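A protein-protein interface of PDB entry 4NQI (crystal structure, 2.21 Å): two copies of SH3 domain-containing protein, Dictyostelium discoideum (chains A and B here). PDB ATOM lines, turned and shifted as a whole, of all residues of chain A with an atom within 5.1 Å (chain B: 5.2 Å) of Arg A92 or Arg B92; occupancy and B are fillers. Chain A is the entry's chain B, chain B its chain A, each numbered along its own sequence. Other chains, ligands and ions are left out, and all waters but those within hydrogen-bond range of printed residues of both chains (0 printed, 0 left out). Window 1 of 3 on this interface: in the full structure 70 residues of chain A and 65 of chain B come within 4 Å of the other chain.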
ATOM      1  N   TYR A  45     -10.368 -25.794 -25.049  1.00  0.00           N
ATOM      2  CA  TYR A  45      -9.129 -25.361 -25.685  1.00  0.00           C
ATOM      3  C   TYR A  45      -9.145 -23.851 -25.892  1.00  0.00           C
ATOM      4  O   TYR A  45      -8.157 -23.166 -25.617  1.00  0.00           O
ATOM      5  CB  TYR A  45      -8.944 -26.079 -27.026  1.00  0.00           C
ATOM      6  CG  TYR A  45      -7.646 -25.767 -27.742  1.00  0.00           C
ATOM      7  CD1 TYR A  45      -6.480 -26.448 -27.429  1.00  0.00           C
ATOM      8  CD2 TYR A  45      -7.592 -24.808 -28.743  1.00  0.00           C
ATOM      9  CE1 TYR A  45      -5.292 -26.175 -28.082  1.00  0.00           C
ATOM     10  CE2 TYR A  45      -6.407 -24.527 -29.402  1.00  0.00           C
ATOM     11  CZ  TYR A  45      -5.262 -25.214 -29.066  1.00  0.00           C
ATOM     12  OH  TYR A  45      -4.080 -24.944 -29.715  1.00  0.00           O
ATOM     13  N   ALA A  49      -6.740 -20.918 -24.253  1.00  0.00           N
ATOM     14  CA  ALA A  49      -6.021 -20.012 -25.146  1.00  0.00           C
ATOM     15  C   ALA A  49      -6.159 -18.566 -24.676  1.00  0.00           C
ATOM     16  O   ALA A  49      -5.184 -17.808 -24.676  1.00  0.00           O
ATOM     17  CB  ALA A  49      -6.522 -20.160 -26.572  1.00  0.00           C
ATOM     18  N   LEU A  52      -3.965 -18.129 -21.575  1.00  0.00           N
ATOM     19  CA  LEU A  52      -2.580 -17.927 -21.986  1.00  0.00           C
ATOM     20  C   LEU A  52      -2.378 -16.519 -22.541  1.00  0.00           C
ATOM     21  O   LEU A  52      -1.338 -15.899 -22.315  1.00  0.00           O
ATOM     22  CB  LEU A  52      -2.174 -18.970 -23.031  1.00  0.00           C
ATOM     23  CG  LEU A  52      -0.742 -18.880 -23.563  1.00  0.00           C
ATOM     24  CD1 LEU A  52       0.262 -19.034 -22.431  1.00  0.00           C
ATOM     25  CD2 LEU A  52      -0.491 -19.919 -24.651  1.00  0.00           C
ATOM     26  N   SER A  53      -3.378 -16.017 -23.262  1.00  0.00           N
ATOM     27  CA  SER A  53      -3.330 -14.665 -23.813  1.00  0.00           C
ATOM     28  C   SER A  53      -3.201 -13.611 -22.714  1.00  0.00           C
ATOM     29  O   SER A  53      -2.349 -12.722 -22.789  1.00  0.00           O
ATOM     30  CB  SER A  53      -4.576 -14.396 -24.656  1.00  0.00           C
ATOM     31  OG  SER A  53      -4.615 -13.053 -25.098  1.00  0.00           O
ATOM     32  N   LEU A  88       1.226  -9.954 -30.132  1.00  0.00           N
ATOM     33  CA  LEU A  88       1.027 -11.371 -30.433  1.00  0.00           C
ATOM     34  C   LEU A  88      -0.020 -12.028 -29.526  1.00  0.00           C
ATOM     35  O   LEU A  88      -0.813 -12.852 -29.986  1.00  0.00           O
ATOM     36  CB  LEU A  88       2.354 -12.130 -30.357  1.00  0.00           C
ATOM     37  CG  LEU A  88       3.369 -11.809 -31.458  1.00  0.00           C
ATOM     38  CD1 LEU A  88       4.683 -12.531 -31.218  1.00  0.00           C
ATOM     39  CD2 LEU A  88       2.815 -12.178 -32.824  1.00  0.00           C
ATOM     40  N   GLU A  89      -0.031 -11.663 -28.247  1.00  0.00           N
ATOM     41  CA  GLU A  89      -0.999 -12.236 -27.313  1.00  0.00           C
ATOM     42  C   GLU A  89      -2.412 -11.714 -27.563  1.00  0.00           C
ATOM     43  O   GLU A  89      -3.391 -12.431 -27.342  1.00  0.00           O
ATOM     44  CB  GLU A  89      -0.582 -12.000 -25.857  1.00  0.00           C
ATOM     45  CG  GLU A  89       0.697 -12.724 -25.447  1.00  0.00           C
ATOM     46  CD  GLU A  89       0.666 -14.217 -25.749  1.00  0.00           C
ATOM     47  OE1 GLU A  89      -0.412 -14.840 -25.638  1.00  0.00           O
ATOM     48  OE2 GLU A  89       1.729 -14.770 -26.099  1.00  0.00           O
ATOM     49  N   ASN A  90      -2.515 -10.470 -28.023  1.00  0.00           N
ATOM     50  CA  ASN A  90      -3.798  -9.928 -28.456  1.00  0.00           C
ATOM     51  C   ASN A  90      -4.342 -10.714 -29.647  1.00  0.00           C
ATOM     52  O   ASN A  90      -5.541 -10.988 -29.726  1.00  0.00           O
ATOM     53  CB  ASN A  90      -3.671  -8.441 -28.815  1.00  0.00           C
ATOM     54  CG  ASN A  90      -3.826  -7.527 -27.608  1.00  0.00           C
ATOM     55  OD1 ASN A  90      -4.657  -7.767 -26.731  1.00  0.00           O
ATOM     56  ND2 ASN A  90      -3.027  -6.467 -27.567  1.00  0.00           N
ATOM     57  N   ARG A  91      -3.453 -11.084 -30.565  1.00  0.00           N
ATOM     58  CA  ARG A  91      -3.851 -11.826 -31.758  1.00  0.00           C
ATOM     59  C   ARG A  91      -4.171 -13.288 -31.457  1.00  0.00           C
ATOM     60  O   ARG A  91      -4.962 -13.911 -32.167  1.00  0.00           O
ATOM     61  CB  ARG A  91      -2.778 -11.725 -32.844  1.00  0.00           C
ATOM     62  CG  ARG A  91      -2.490 -10.297 -33.291  1.00  0.00           C
ATOM     63  CD  ARG A  91      -1.471 -10.251 -34.422  1.00  0.00           C
ATOM     64  NE  ARG A  91      -0.786  -8.961 -34.484  1.00  0.00           N
ATOM     65  CZ  ARG A  91      -0.570  -8.271 -35.600  1.00  0.00           C
ATOM     66  NH1 ARG A  91      -0.988  -8.738 -36.769  1.00  0.00           N
ATOM     67  NH2 ARG A  91       0.066  -7.107 -35.546  1.00  0.00           N
ATOM     68  N   ARG A  92      -3.557 -13.839 -30.411  1.00  0.00           N
ATOM     69  CA  ARG A  92      -3.891 -15.193 -29.982  1.00  0.00           C
ATOM     70  C   ARG A  92      -5.323 -15.210 -29.465  1.00  0.00           C
ATOM     71  O   ARG A  92      -6.066 -16.164 -29.700  1.00  0.00           O
ATOM     72  CB  ARG A  92      -2.941 -15.694 -28.892  1.00  0.00           C
ATOM     73  CG  ARG A  92      -3.156 -17.165 -28.537  1.00  0.00           C
ATOM     74  CD  ARG A  92      -2.495 -17.556 -27.221  1.00  0.00           C
ATOM     75  NE  ARG A  92      -1.100 -17.131 -27.158  1.00  0.00           N
ATOM     76  CZ  ARG A  92      -0.088 -17.804 -27.698  1.00  0.00           C
ATOM     77  NH1 ARG A  92      -0.313 -18.936 -28.351  1.00  0.00           N
ATOM     78  NH2 ARG A  92       1.150 -17.341 -27.589  1.00  0.00           N
ATOM     79  N   ASP A  93      -5.706 -14.143 -28.768  1.00  0.00           N
ATOM     80  CA  ASP A  93      -7.072 -14.000 -28.280  1.00  0.00           C
ATOM     81  C   ASP A  93      -8.064 -13.991 -29.446  1.00  0.00           C
ATOM     82  O   ASP A  93      -9.105 -14.656 -29.389  1.00  0.00           O
ATOM     83  CB  ASP A  93      -7.210 -12.729 -27.442  1.00  0.00           C
ATOM     84  CG  ASP A  93      -8.610 -12.537 -26.898  1.00  0.00           C
ATOM     85  OD1 ASP A  93      -9.032 -13.342 -26.039  1.00  0.00           O
ATOM     86  OD2 ASP A  93      -9.287 -11.575 -27.320  1.00  0.00           O
ATOM     87  N   ASP A  94      -7.729 -13.255 -30.503  1.00  0.00           N
ATOM     88  CA  ASP A  94      -8.563 -13.204 -31.702  1.00  0.00           C
ATOM     89  C   ASP A  94      -8.683 -14.579 -32.355  1.00  0.00           C
ATOM     90  O   ASP A  94      -9.733 -14.929 -32.898  1.00  0.00           O
ATOM     91  CB  ASP A  94      -8.005 -12.190 -32.702  1.00  0.00           C
ATOM     92  CG  ASP A  94      -8.119 -10.758 -32.208  1.00  0.00           C
ATOM     93  OD1 ASP A  94      -8.930 -10.501 -31.290  1.00  0.00           O
ATOM     94  OD2 ASP A  94      -7.403  -9.887 -32.747  1.00  0.00           O
ATOM     95  N   VAL A  95      -7.599 -15.351 -32.303  1.00  0.00           N
ATOM     96  CA  VAL A  95      -7.606 -16.725 -32.795  1.00  0.00           C
ATOM     97  C   VAL A  95      -8.612 -17.571 -32.012  1.00  0.00           C
ATOM     98  O   VAL A  95      -9.409 -18.308 -32.596  1.00  0.00           O
ATOM     99  CB  VAL A  95      -6.200 -17.355 -32.722  1.00  0.00           C
ATOM    100  CG1 VAL A  95      -6.267 -18.862 -32.909  1.00  0.00           C
ATOM    101  CG2 VAL A  95      -5.284 -16.729 -33.767  1.00  0.00           C
ATOM    102  N   ALA A  96      -8.586 -17.443 -30.688  1.00  0.00           N
ATOM    103  CA  ALA A  96      -9.529 -18.155 -29.827  1.00  0.00           C
ATOM    104  C   ALA A  96     -10.978 -17.790 -30.159  1.00  0.00           C
ATOM    105  O   ALA A  96     -11.854 -18.659 -30.198  1.00  0.00           O
ATOM    106  CB  ALA A  96      -9.231 -17.864 -28.366  1.00  0.00           C
ATOM    107  N   GLU A 202      -4.531 -19.728 -37.186  1.00  0.00           N
ATOM    108  CA  GLU A 202      -3.350 -20.249 -36.497  1.00  0.00           C
ATOM    109  C   GLU A 202      -2.100 -20.051 -37.343  1.00  0.00           C
ATOM    110  O   GLU A 202      -1.053 -19.640 -36.836  1.00  0.00           O
ATOM    111  CB  GLU A 202      -3.510 -21.734 -36.166  1.00  0.00           C
ATOM    112  CG  GLU A 202      -4.250 -22.027 -34.872  1.00  0.00           C
ATOM    113  CD  GLU A 202      -3.419 -21.752 -33.628  1.00  0.00           C
ATOM    114  OE1 GLU A 202      -2.345 -21.121 -33.742  1.00  0.00           O
ATOM    115  OE2 GLU A 202      -3.845 -22.171 -32.532  1.00  0.00           O
ATOM    116  N   LEU A 205      -1.178 -16.330 -37.218  1.00  0.00           N
ATOM    117  CA  LEU A 205      -0.512 -16.000 -35.959  1.00  0.00           C
ATOM    118  C   LEU A 205       0.930 -16.497 -35.947  1.00  0.00           C
ATOM    119  O   LEU A 205       1.841 -15.770 -35.540  1.00  0.00           O
ATOM    120  CB  LEU A 205      -1.268 -16.595 -34.770  1.00  0.00           C
ATOM    121  CG  LEU A 205      -0.553 -16.446 -33.423  1.00  0.00           C
ATOM    122  CD1 LEU A 205      -0.567 -14.999 -32.961  1.00  0.00           C
ATOM    123  CD2 LEU A 205      -1.157 -17.346 -32.362  1.00  0.00           C
ATOM    124  N   TYR B  45       2.944 -17.686 -17.309  1.00  0.00           N
ATOM    125  CA  TYR B  45       2.772 -17.863 -18.748  1.00  0.00           C
ATOM    126  C   TYR B  45       3.060 -19.308 -19.123  1.00  0.00           C
ATOM    127  O   TYR B  45       2.277 -19.947 -19.825  1.00  0.00           O
ATOM    128  CB  TYR B  45       3.706 -16.924 -19.516  1.00  0.00           C
ATOM    129  CG  TYR B  45       3.492 -16.916 -21.014  1.00  0.00           C
ATOM    130  CD1 TYR B  45       2.449 -16.194 -21.579  1.00  0.00           C
ATOM    131  CD2 TYR B  45       4.339 -17.615 -21.865  1.00  0.00           C
ATOM    132  CE1 TYR B  45       2.249 -16.176 -22.945  1.00  0.00           C
ATOM    133  CE2 TYR B  45       4.147 -17.603 -23.235  1.00  0.00           C
ATOM    134  CZ  TYR B  45       3.099 -16.881 -23.768  1.00  0.00           C
ATOM    135  OH  TYR B  45       2.897 -16.863 -25.128  1.00  0.00           O
ATOM    136  N   ALA B  49       0.614 -22.240 -20.731  1.00  0.00           N
ATOM    137  CA  ALA B  49       1.033 -22.888 -21.969  1.00  0.00           C
ATOM    138  C   ALA B  49       0.932 -24.408 -21.857  1.00  0.00           C
ATOM    139  O   ALA B  49       0.624 -25.087 -22.838  1.00  0.00           O
ATOM    140  CB  ALA B  49       2.448 -22.475 -22.329  1.00  0.00           C
ATOM    141  N   LEU B  52      -2.906 -25.210 -21.887  1.00  0.00           N
ATOM    142  CA  LEU B  52      -3.353 -25.157 -23.275  1.00  0.00           C
ATOM    143  C   LEU B  52      -2.909 -26.406 -24.031  1.00  0.00           C
ATOM    144  O   LEU B  52      -3.679 -26.977 -24.804  1.00  0.00           O
ATOM    145  CB  LEU B  52      -2.816 -23.904 -23.971  1.00  0.00           C
ATOM    146  CG  LEU B  52      -3.224 -23.756 -25.440  1.00  0.00           C
ATOM    147  CD1 LEU B  52      -4.741 -23.741 -25.566  1.00  0.00           C
ATOM    148  CD2 LEU B  52      -2.620 -22.506 -26.062  1.00  0.00           C
ATOM    149  N   SER B  53      -1.668 -26.824 -23.799  1.00  0.00           N
ATOM    150  CA  SER B  53      -1.128 -28.029 -24.423  1.00  0.00           C
ATOM    151  C   SER B  53      -1.951 -29.268 -24.064  1.00  0.00           C
ATOM    152  O   SER B  53      -2.253 -30.096 -24.928  1.00  0.00           O
ATOM    153  CB  SER B  53       0.332 -28.222 -24.012  1.00  0.00           C
ATOM    154  OG  SER B  53       0.857 -29.429 -24.535  1.00  0.00           O
ATOM    155  N   LEU B  88       1.857 -30.917 -32.516  1.00  0.00           N
ATOM    156  CA  LEU B  88       2.047 -29.492 -32.258  1.00  0.00           C
ATOM    157  C   LEU B  88       1.862 -29.131 -30.787  1.00  0.00           C
ATOM    158  O   LEU B  88       2.621 -28.328 -30.238  1.00  0.00           O
ATOM    159  CB  LEU B  88       1.103 -28.659 -33.127  1.00  0.00           C
ATOM    160  CG  LEU B  88       1.384 -28.720 -34.630  1.00  0.00           C
ATOM    161  CD1 LEU B  88       0.389 -27.873 -35.406  1.00  0.00           C
ATOM    162  CD2 LEU B  88       2.807 -28.272 -34.928  1.00  0.00           C
ATOM    163  N   GLU B  89       0.856 -29.721 -30.151  1.00  0.00           N
ATOM    164  CA  GLU B  89       0.591 -29.420 -28.750  1.00  0.00           C
ATOM    165  C   GLU B  89       1.647 -30.038 -27.837  1.00  0.00           C
ATOM    166  O   GLU B  89       1.902 -29.530 -26.741  1.00  0.00           O
ATOM    167  CB  GLU B  89      -0.821 -29.854 -28.352  1.00  0.00           C
ATOM    168  CG  GLU B  89      -1.929 -29.042 -29.026  1.00  0.00           C
ATOM    169  CD  GLU B  89      -1.783 -27.539 -28.816  1.00  0.00           C
ATOM    170  OE1 GLU B  89      -1.275 -27.117 -27.752  1.00  0.00           O
ATOM    171  OE2 GLU B  89      -2.183 -26.773 -29.718  1.00  0.00           O
ATOM    172  N   ASN B  90       2.267 -31.123 -28.292  1.00  0.00           N
ATOM    173  CA  ASN B  90       3.419 -31.676 -27.591  1.00  0.00           C
ATOM    174  C   ASN B  90       4.630 -30.764 -27.741  1.00  0.00           C
ATOM    175  O   ASN B  90       5.450 -30.651 -26.828  1.00  0.00           O
ATOM    176  CB  ASN B  90       3.747 -33.086 -28.087  1.00  0.00           C
ATOM    177  CG  ASN B  90       2.900 -34.151 -27.417  1.00  0.00           C
ATOM    178  OD1 ASN B  90       2.338 -33.932 -26.342  1.00  0.00           O
ATOM    179  ND2 ASN B  90       2.811 -35.317 -28.047  1.00  0.00           N
ATOM    180  N   ARG B  91       4.739 -30.110 -28.893  1.00  0.00           N
ATOM    181  CA  ARG B  91       5.828 -29.166 -29.115  1.00  0.00           C
ATOM    182  C   ARG B  91       5.607 -27.887 -28.315  1.00  0.00           C
ATOM    183  O   ARG B  91       6.566 -27.233 -27.903  1.00  0.00           O
ATOM    184  CB  ARG B  91       6.008 -28.848 -30.599  1.00  0.00           C
ATOM    185  CG  ARG B  91       7.402 -28.338 -30.922  1.00  0.00           C
ATOM    186  CD  ARG B  91       7.586 -28.021 -32.395  1.00  0.00           C
ATOM    187  NE  ARG B  91       8.964 -28.270 -32.811  1.00  0.00           N
ATOM    188  CZ  ARG B  91       9.381 -29.419 -33.330  1.00  0.00           C
ATOM    189  NH1 ARG B  91       8.516 -30.407 -33.519  1.00  0.00           N
ATOM    190  NH2 ARG B  91      10.648 -29.574 -33.686  1.00  0.00           N
ATOM    191  N   ARG B  92       4.343 -27.529 -28.100  1.00  0.00           N
ATOM    192  CA  ARG B  92       4.045 -26.370 -27.268  1.00  0.00           C
ATOM    193  C   ARG B  92       4.539 -26.627 -25.850  1.00  0.00           C
ATOM    194  O   ARG B  92       5.042 -25.715 -25.196  1.00  0.00           O
ATOM    195  CB  ARG B  92       2.553 -26.028 -27.257  1.00  0.00           C
ATOM    196  CG  ARG B  92       2.254 -24.692 -26.576  1.00  0.00           C
ATOM    197  CD  ARG B  92       0.768 -24.477 -26.295  1.00  0.00           C
ATOM    198  NE  ARG B  92      -0.063 -24.694 -27.475  1.00  0.00           N
ATOM    199  CZ  ARG B  92      -0.208 -23.817 -28.464  1.00  0.00           C
ATOM    200  NH1 ARG B  92       0.434 -22.656 -28.427  1.00  0.00           N
ATOM    201  NH2 ARG B  92      -0.990 -24.103 -29.496  1.00  0.00           N
ATOM    202  N   ASP B  93       4.425 -27.872 -25.392  1.00  0.00           N
ATOM    203  CA  ASP B  93       4.889 -28.247 -24.061  1.00  0.00           C
ATOM    204  C   ASP B  93       6.411 -28.139 -23.970  1.00  0.00           C
ATOM    205  O   ASP B  93       6.940 -27.684 -22.954  1.00  0.00           O
ATOM    206  CB  ASP B  93       4.423 -29.659 -23.695  1.00  0.00           C
ATOM    207  CG  ASP B  93       4.726 -30.020 -22.253  1.00  0.00           C
ATOM    208  OD1 ASP B  93       3.924 -29.662 -21.362  1.00  0.00           O
ATOM    209  OD2 ASP B  93       5.766 -30.667 -22.009  1.00  0.00           O
ATOM    210  N   ASP B  94       7.109 -28.535 -25.036  1.00  0.00           N
ATOM    211  CA  ASP B  94       8.561 -28.368 -25.105  1.00  0.00           C
ATOM    212  C   ASP B  94       8.946 -26.898 -24.953  1.00  0.00           C
ATOM    213  O   ASP B  94       9.875 -26.566 -24.212  1.00  0.00           O
ATOM    214  CB  ASP B  94       9.118 -28.905 -26.428  1.00  0.00           C
ATOM    215  CG  ASP B  94       9.059 -30.421 -26.520  1.00  0.00           C
ATOM    216  OD1 ASP B  94       8.773 -31.077 -25.493  1.00  0.00           O
ATOM    217  OD2 ASP B  94       9.312 -30.958 -27.621  1.00  0.00           O
ATOM    218  N   VAL B  95       8.231 -26.028 -25.663  1.00  0.00           N
ATOM    219  CA  VAL B  95       8.465 -24.587 -25.606  1.00  0.00           C
ATOM    220  C   VAL B  95       8.349 -24.062 -24.177  1.00  0.00           C
ATOM    221  O   VAL B  95       9.217 -23.328 -23.707  1.00  0.00           O
ATOM    222  CB  VAL B  95       7.482 -23.823 -26.514  1.00  0.00           C
ATOM    223  CG1 VAL B  95       7.534 -22.337 -26.226  1.00  0.00           C
ATOM    224  CG2 VAL B  95       7.791 -24.093 -27.983  1.00  0.00           C
ATOM    225  N   ALA B  96       7.281 -24.454 -23.489  1.00  0.00           N
ATOM    226  CA  ALA B  96       7.066 -24.056 -22.102  1.00  0.00           C
ATOM    227  C   ALA B  96       8.216 -24.504 -21.194  1.00  0.00           C
ATOM    228  O   ALA B  96       8.593 -23.786 -20.263  1.00  0.00           O
ATOM    229  CB  ALA B  96       5.740 -24.603 -21.596  1.00  0.00           C
ATOM    230  N   GLU B 202       9.778 -20.590 -29.880  1.00  0.00           N
ATOM    231  CA  GLU B 202       8.490 -20.104 -30.362  1.00  0.00           C
ATOM    232  C   GLU B 202       8.505 -20.034 -31.885  1.00  0.00           C
ATOM    233  O   GLU B 202       7.538 -20.417 -32.541  1.00  0.00           O
ATOM    234  CB  GLU B 202       8.170 -18.728 -29.773  1.00  0.00           C
ATOM    235  CG  GLU B 202       7.262 -18.773 -28.556  1.00  0.00           C
ATOM    236  CD  GLU B 202       5.989 -19.560 -28.810  1.00  0.00           C
ATOM    237  OE1 GLU B 202       5.069 -19.022 -29.462  1.00  0.00           O
ATOM    238  OE2 GLU B 202       5.910 -20.722 -28.364  1.00  0.00           O
ATOM    239  N   LEU B 205       8.298 -23.554 -33.245  1.00  0.00           N
ATOM    240  CA  LEU B 205       6.919 -24.024 -33.133  1.00  0.00           C
ATOM    241  C   LEU B 205       6.024 -23.398 -34.202  1.00  0.00           C
ATOM    242  O   LEU B 205       5.143 -24.065 -34.753  1.00  0.00           O
ATOM    243  CB  LEU B 205       6.361 -23.724 -31.738  1.00  0.00           C
ATOM    244  CG  LEU B 205       4.854 -23.902 -31.517  1.00  0.00           C
ATOM    245  CD1 LEU B 205       4.416 -25.320 -31.836  1.00  0.00           C
ATOM    246  CD2 LEU B 205       4.460 -23.538 -30.091  1.00  0.00           C
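Arg B92 touches just these residues of chain A: Tyr A45 and Arg A92.
Printed residues of chain A within 4 Å of Tyr B45: Leu A52 (3.4 Å), Glu A89 (2.6 Å) and Arg A92 (3.1 Å).
Printed residues of chain A within 4 Å of Ala B49: Leu A52 (3.6 Å).
Printed residues of chain B within 4 Å of Glu A89: Tyr B45.
Of the printed residues of chain B, Tyr A45 touches Leu B52, Glu B89 and Arg B92.
Of the printed residues of chain A, Glu B89 touches Tyr A45 (2.6 Å).
Asp B93 touches none of the printed residues of chain A.
The nearest residue of chain A that does not touch Arg B92 is Glu A202 (4.6 Å).
The side-chain hydroxyl (OH) of Tyr B45 lies within hydrogen-bond range of the side-chain carboxylate (OE2) of Glu A89, at 2.6 Å.
The guanidinium group of Arg A92 is in hydrogen-bond range of the side-chain hydroxyl of Tyr B45.
OE2 of Glu B89 sits at hydrogen-bond distance from OH of Tyr A45.
OH of Tyr A45 is in hydrogen-bond range of NH2 of Arg B92.
The side-chain hydroxyl (OG) of Ser B53 sits at hydrogen-bond distance from the backbone carbonyl oxygen (O) of Glu B89 (2.4 Å).
The guanidinium group (NE) of Arg B92 is in salt-bridge range of the side-chain carboxylate (OE1) of Glu B89, 2.7 Å away.
The side-chain hydroxyl (OG) of Ser A53 sits at hydrogen-bond distance from the backbone carbonyl oxygen (O) of Glu A89 (2.6 Å).
The side-chain carboxylate (OE1) of Glu A89 lies within salt-bridge range of the guanidinium group (NE) of Arg A92 (2.8 Å).
Among the printed residues, merely in contact across the chains: Tyr A45 with Leu B52, Ala A49 with Leu B52, Leu A52 with Tyr B45, Leu A52 with Ala B49, Leu A52 with Leu B52 and Arg A92 with Arg B92.
Of the 15 printed residues of chain B, 5 touch a printed residue of chain A.
Printed residues of chain A that touch a printed residue of chain B: Tyr A45, Ala A49, Leu A52, Glu A89 and Arg A92.
Hydrophobic or aromatic side chains of chain A that line the printed part of chain B: Tyr A45 and Leu A52.
Among the printed residues, no Asp or Glu carboxylate lies within 4 Å of a Lys or Arg side-chain nitrogen of the other chain.
Tyr A45 touches Leu B52, and with the chains exchanged Leu A52 touches Tyr B45.
Tyr A45 touches Glu B89, and with the chains exchanged Glu A89 touches Tyr B45.
Tyr A45 touches Arg B92, and with the chains exchanged Arg A92 touches Tyr B45.
Leu B52 touches its own counterpart, Leu A52.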
